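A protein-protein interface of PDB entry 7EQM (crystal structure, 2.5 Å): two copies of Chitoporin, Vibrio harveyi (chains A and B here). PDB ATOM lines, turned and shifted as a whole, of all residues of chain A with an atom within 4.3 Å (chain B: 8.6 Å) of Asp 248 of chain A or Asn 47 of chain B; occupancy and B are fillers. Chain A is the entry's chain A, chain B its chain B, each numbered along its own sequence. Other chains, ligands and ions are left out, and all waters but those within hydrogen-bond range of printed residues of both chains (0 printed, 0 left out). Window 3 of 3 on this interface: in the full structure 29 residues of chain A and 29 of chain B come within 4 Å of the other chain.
Of the printed residues of chain B, Phe 283 of chain A touches Asn 47.
Of the printed residues of chain B, Val 284 of chain A touches Phe 45 (3.5 Å), Ala 46 (3.6 Å), Asn 47 (2.9 Å) and Phe 48 (3.4 Å).
Of the printed residues of chain A, Phe 45 of chain B touches Val 284.
Printed residues of chain A within 4 Å of Ala 46 of chain B: Val 284 (3.6 Å).
Of the printed residues of chain A, Phe 48 of chain B touches Val 284 (3.4 Å).
The nearest printed residue of chain A that does not touch Asn 47 of chain B is Gly 247 of chain A (7.7 Å).
The backbone NH (N) of Phe 283 of chain A sits at hydrogen-bond distance from the backbone carbonyl oxygen (O) of Asp 248 of chain A, 2.8 Å away.
The side-chain amide nitrogen (NE2) of Gln 44 of chain B lies within hydrogen-bond range of the backbone carbonyl oxygen (O) of Phe 48 of chain B (2.9 Å).
Printed residues of chain A that touch a printed residue of chain B: Asp 248, Tyr 282, Phe 283 and Val 284.
Hydrophobic or aromatic side chains of chain A that line the printed part of chain B: Tyr 282 and Val 284.
No position is printed for both chains.
Of the 7 pairs that touch across the chains among the printed residues, none has its exchanged pair printed and touching as well.
The backbone carbonyl oxygen (O) of Phe 283 of chain A sits at hydrogen-bond distance from the side-chain amide nitrogen (ND2) of Asn 47 of chain B (2.9 Å).
The backbone carbonyl oxygen (O) of Val 284 of chain A lies within hydrogen-bond range of the backbone NH (N) of Asn 47 of chain B, 2.9 Å away.
OD2 of Asp 248 of chain A touches ND2 of Asn 47 of chain B, 3.6 Å away.
Tyr 282 of chain A touches Asn 47 of chain B (OH to CB, 3.2 Å).
Val 284 of chain A touches Phe 45 of chain B (CG1 to CD2, 3.5 Å).
N of Ala 46 of chain B touches O of Val 284 of chain A, at 3.6 Å.
Phe 48 of chain B touches Val 284 of chain A.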
ATOM      1  N   THR A 246       9.370  20.930  20.313  1.00  0.00           N
ATOM      2  CA  THR A 246       9.913  22.087  21.005  1.00  0.00           C
ATOM      3  C   THR A 246       9.120  23.316  20.584  1.00  0.00           C
ATOM      4  O   THR A 246       8.979  23.597  19.391  1.00  0.00           O
ATOM      5  CB  THR A 246      11.414  22.247  20.711  1.00  0.00           C
ATOM      6  OG1 THR A 246      11.907  23.422  21.359  1.00  0.00           O
ATOM      7  CG2 THR A 246      11.700  22.305  19.197  1.00  0.00           C
ATOM      8  N   GLY A 247       8.584  24.033  21.564  1.00  0.00           N
ATOM      9  CA  GLY A 247       7.803  25.220  21.261  1.00  0.00           C
ATOM     10  C   GLY A 247       6.574  24.909  20.430  1.00  0.00           C
ATOM     11  O   GLY A 247       5.737  24.087  20.820  1.00  0.00           O
ATOM     12  N   ASP A 248       6.460  25.546  19.272  1.00  0.00           N
ATOM     13  CA  ASP A 248       5.326  25.324  18.391  1.00  0.00           C
ATOM     14  C   ASP A 248       5.638  24.332  17.277  1.00  0.00           C
ATOM     15  O   ASP A 248       4.876  24.243  16.312  1.00  0.00           O
ATOM     16  CB  ASP A 248       4.854  26.659  17.805  1.00  0.00           C
ATOM     17  CG  ASP A 248       4.195  27.537  18.842  1.00  0.00           C
ATOM     18  OD1 ASP A 248       3.570  26.975  19.763  1.00  0.00           O
ATOM     19  OD2 ASP A 248       4.291  28.778  18.741  1.00  0.00           O
ATOM     20  N   TRP A 249       6.728  23.578  17.394  1.00  0.00           N
ATOM     21  CA  TRP A 249       7.205  22.718  16.321  1.00  0.00           C
ATOM     22  C   TRP A 249       7.321  21.272  16.778  1.00  0.00           C
ATOM     23  O   TRP A 249       7.639  20.992  17.942  1.00  0.00           O
ATOM     24  CB  TRP A 249       8.563  23.178  15.829  1.00  0.00           C
ATOM     25  CG  TRP A 249       8.523  24.549  15.329  1.00  0.00           C
ATOM     26  CD1 TRP A 249       8.677  25.697  16.052  1.00  0.00           C
ATOM     27  CD2 TRP A 249       8.291  24.945  13.977  1.00  0.00           C
ATOM     28  NE1 TRP A 249       8.560  26.785  15.225  1.00  0.00           N
ATOM     29  CE2 TRP A 249       8.328  26.351  13.945  1.00  0.00           C
ATOM     30  CE3 TRP A 249       8.062  24.245  12.791  1.00  0.00           C
ATOM     31  CZ2 TRP A 249       8.152  27.072  12.768  1.00  0.00           C
ATOM     32  CZ3 TRP A 249       7.878  24.958  11.631  1.00  0.00           C
ATOM     33  CH2 TRP A 249       7.931  26.360  11.624  1.00  0.00           C
ATOM     34  N   MET A 281       6.110  19.818  11.643  1.00  0.00           N
ATOM     35  CA  MET A 281       4.750  20.252  11.931  1.00  0.00           C
ATOM     36  C   MET A 281       4.770  21.501  12.808  1.00  0.00           C
ATOM     37  O   MET A 281       5.556  21.601  13.756  1.00  0.00           O
ATOM     38  CB  MET A 281       3.938  19.146  12.615  1.00  0.00           C
ATOM     39  CG  MET A 281       2.462  19.514  12.868  1.00  0.00           C
ATOM     40  SD  MET A 281       1.349  18.105  13.180  1.00  0.00           S
ATOM     41  CE  MET A 281       2.124  17.303  14.593  1.00  0.00           C
ATOM     42  N   TYR A 282       3.874  22.433  12.502  1.00  0.00           N
ATOM     43  CA  TYR A 282       3.778  23.717  13.183  1.00  0.00           C
ATOM     44  C   TYR A 282       2.400  23.846  13.814  1.00  0.00           C
ATOM     45  O   TYR A 282       1.383  23.820  13.110  1.00  0.00           O
ATOM     46  CB  TYR A 282       4.009  24.866  12.207  1.00  0.00           C
ATOM     47  CG  TYR A 282       4.030  26.203  12.855  1.00  0.00           C
ATOM     48  CD1 TYR A 282       4.968  26.496  13.842  1.00  0.00           C
ATOM     49  CD2 TYR A 282       3.127  27.197  12.477  1.00  0.00           C
ATOM     50  CE1 TYR A 282       5.011  27.751  14.446  1.00  0.00           C
ATOM     51  CE2 TYR A 282       3.163  28.463  13.066  1.00  0.00           C
ATOM     52  CZ  TYR A 282       4.108  28.727  14.051  1.00  0.00           C
ATOM     53  OH  TYR A 282       4.156  29.959  14.651  1.00  0.00           O
ATOM     54  N   PHE A 283       2.378  24.023  15.134  1.00  0.00           N
ATOM     55  CA  PHE A 283       1.150  24.185  15.909  1.00  0.00           C
ATOM     56  C   PHE A 283       0.635  25.597  15.698  1.00  0.00           C
ATOM     57  O   PHE A 283       0.780  26.482  16.545  1.00  0.00           O
ATOM     58  CB  PHE A 283       1.416  23.891  17.373  1.00  0.00           C
ATOM     59  CG  PHE A 283       1.929  22.523  17.588  1.00  0.00           C
ATOM     60  CD1 PHE A 283       1.282  21.442  16.995  1.00  0.00           C
ATOM     61  CD2 PHE A 283       3.070  22.300  18.339  1.00  0.00           C
ATOM     62  CE1 PHE A 283       1.754  20.154  17.169  1.00  0.00           C
ATOM     63  CE2 PHE A 283       3.551  21.015  18.532  1.00  0.00           C
ATOM     64  CZ  PHE A 283       2.897  19.939  17.943  1.00  0.00           C
ATOM     65  N   VAL A 284       0.005  25.799  14.537  1.00  0.00           N
ATOM     66  CA  VAL A 284      -0.373  27.142  14.134  1.00  0.00           C
ATOM     67  C   VAL A 284      -1.502  27.702  15.004  1.00  0.00           C
ATOM     68  O   VAL A 284      -1.687  28.925  15.067  1.00  0.00           O
ATOM     69  CB  VAL A 284      -0.734  27.119  12.633  1.00  0.00           C
ATOM     70  CG1 VAL A 284      -2.107  26.472  12.395  1.00  0.00           C
ATOM     71  CG2 VAL A 284      -0.662  28.519  12.038  1.00  0.00           C
ATOM     72  N   GLN B  44      -9.312  32.440  12.722  1.00  0.00           N
ATOM     73  CA  GLN B  44      -8.098  33.244  12.814  1.00  0.00           C
ATOM     74  C   GLN B  44      -7.099  32.470  13.659  1.00  0.00           C
ATOM     75  O   GLN B  44      -7.308  32.291  14.865  1.00  0.00           O
ATOM     76  CB  GLN B  44      -8.393  34.618  13.411  1.00  0.00           C
ATOM     77  CG  GLN B  44      -7.184  35.480  13.599  1.00  0.00           C
ATOM     78  CD  GLN B  44      -6.493  35.791  12.299  1.00  0.00           C
ATOM     79  OE1 GLN B  44      -7.052  36.448  11.425  1.00  0.00           O
ATOM     80  NE2 GLN B  44      -5.262  35.314  12.154  1.00  0.00           N
ATOM     81  N   PHE B  45      -6.037  31.974  13.023  1.00  0.00           N
ATOM     82  CA  PHE B  45      -5.052  31.181  13.747  1.00  0.00           C
ATOM     83  C   PHE B  45      -4.222  32.071  14.662  1.00  0.00           C
ATOM     84  O   PHE B  45      -3.840  33.186  14.292  1.00  0.00           O
ATOM     85  CB  PHE B  45      -4.136  30.446  12.773  1.00  0.00           C
ATOM     86  CG  PHE B  45      -4.801  29.320  12.041  1.00  0.00           C
ATOM     87  CD1 PHE B  45      -5.995  28.789  12.483  1.00  0.00           C
ATOM     88  CD2 PHE B  45      -4.216  28.786  10.905  1.00  0.00           C
ATOM     89  CE1 PHE B  45      -6.593  27.735  11.806  1.00  0.00           C
ATOM     90  CE2 PHE B  45      -4.804  27.740  10.223  1.00  0.00           C
ATOM     91  CZ  PHE B  45      -5.999  27.218  10.667  1.00  0.00           C
ATOM     92  N   ALA B  46      -3.932  31.561  15.861  1.00  0.00           N
ATOM     93  CA  ALA B  46      -3.103  32.302  16.809  1.00  0.00           C
ATOM     94  C   ALA B  46      -1.715  32.628  16.262  1.00  0.00           C
ATOM     95  O   ALA B  46      -1.158  33.669  16.611  1.00  0.00           O
ATOM     96  CB  ALA B  46      -2.968  31.518  18.112  1.00  0.00           C
ATOM     97  N   ASN B  47      -1.137  31.776  15.413  1.00  0.00           N
ATOM     98  CA  ASN B  47       0.249  31.940  14.975  1.00  0.00           C
ATOM     99  C   ASN B  47       0.372  32.120  13.466  1.00  0.00           C
ATOM    100  O   ASN B  47       1.412  31.800  12.883  1.00  0.00           O
ATOM    101  CB  ASN B  47       1.108  30.760  15.423  1.00  0.00           C
ATOM    102  CG  ASN B  47       0.997  30.502  16.906  1.00  0.00           C
ATOM    103  OD1 ASN B  47       0.849  31.427  17.696  1.00  0.00           O
ATOM    104  ND2 ASN B  47       1.052  29.239  17.294  1.00  0.00           N
ATOM    105  N   PHE B  48      -0.680  32.627  12.823  1.00  0.00           N
ATOM    106  CA  PHE B  48      -0.658  32.887  11.387  1.00  0.00           C
ATOM    107  C   PHE B  48      -1.647  34.004  11.092  1.00  0.00           C
ATOM    108  O   PHE B  48      -2.829  33.916  11.445  1.00  0.00           O
ATOM    109  CB  PHE B  48      -1.001  31.623  10.611  1.00  0.00           C
ATOM    110  CG  PHE B  48      -0.553  31.650   9.191  1.00  0.00           C
ATOM    111  CD1 PHE B  48       0.770  31.903   8.878  1.00  0.00           C
ATOM    112  CD2 PHE B  48      -1.468  31.442   8.164  1.00  0.00           C
ATOM    113  CE1 PHE B  48       1.192  31.949   7.554  1.00  0.00           C
ATOM    114  CE2 PHE B  48      -1.068  31.484   6.842  1.00  0.00           C
ATOM    115  CZ  PHE B  48       0.276  31.737   6.532  1.00  0.00           C
ATOM    116  N   GLU B  49      -1.173  35.049  10.453  1.00  0.00           N
ATOM    117  CA  GLU B  49      -2.034  36.210  10.344  1.00  0.00           C
ATOM    118  C   GLU B  49      -3.049  36.099   9.205  1.00  0.00           C
ATOM    119  O   GLU B  49      -4.195  36.498   9.409  1.00  0.00           O
ATOM    120  CB  GLU B  49      -1.214  37.482  10.209  1.00  0.00           C
ATOM    121  CG  GLU B  49      -2.124  38.654  10.067  1.00  0.00           C
ATOM    122  CD  GLU B  49      -2.178  39.211   8.674  1.00  0.00           C
ATOM    123  OE1 GLU B  49      -3.293  39.341   8.110  1.00  0.00           O
ATOM    124  OE2 GLU B  49      -1.089  39.557   8.162  1.00  0.00           O
ATOM    125  N   PRO B  50      -2.725  35.553   8.030  1.00  0.00           N
ATOM    126  CA  PRO B  50      -3.788  35.311   7.044  1.00  0.00           C
ATOM    127  C   PRO B  50      -4.883  34.443   7.647  1.00  0.00           C
ATOM    128  O   PRO B  50      -4.612  33.389   8.222  1.00  0.00           O
ATOM    129  CB  PRO B  50      -3.059  34.600   5.897  1.00  0.00           C
ATOM    130  CG  PRO B  50      -1.643  34.886   6.088  1.00  0.00           C
ATOM    131  CD  PRO B  50      -1.428  35.040   7.549  1.00  0.00           C
ATOM    132  N   PHE B  81      -6.641  30.960   2.623  1.00  0.00           N
ATOM    133  CA  PHE B  81      -6.266  32.058   3.494  1.00  0.00           C
ATOM    134  C   PHE B  81      -6.645  33.362   2.805  1.00  0.00           C
ATOM    135  O   PHE B  81      -6.699  33.439   1.574  1.00  0.00           O
ATOM    136  CB  PHE B  81      -4.767  32.026   3.833  1.00  0.00           C
ATOM    137  CG  PHE B  81      -4.360  30.848   4.688  1.00  0.00           C
ATOM    138  CD1 PHE B  81      -4.554  30.870   6.064  1.00  0.00           C
ATOM    139  CD2 PHE B  81      -3.796  29.717   4.110  1.00  0.00           C
ATOM    140  CE1 PHE B  81      -4.191  29.779   6.850  1.00  0.00           C
ATOM    141  CE2 PHE B  81      -3.435  28.633   4.876  1.00  0.00           C
ATOM    142  CZ  PHE B  81      -3.624  28.660   6.251  1.00  0.00           C
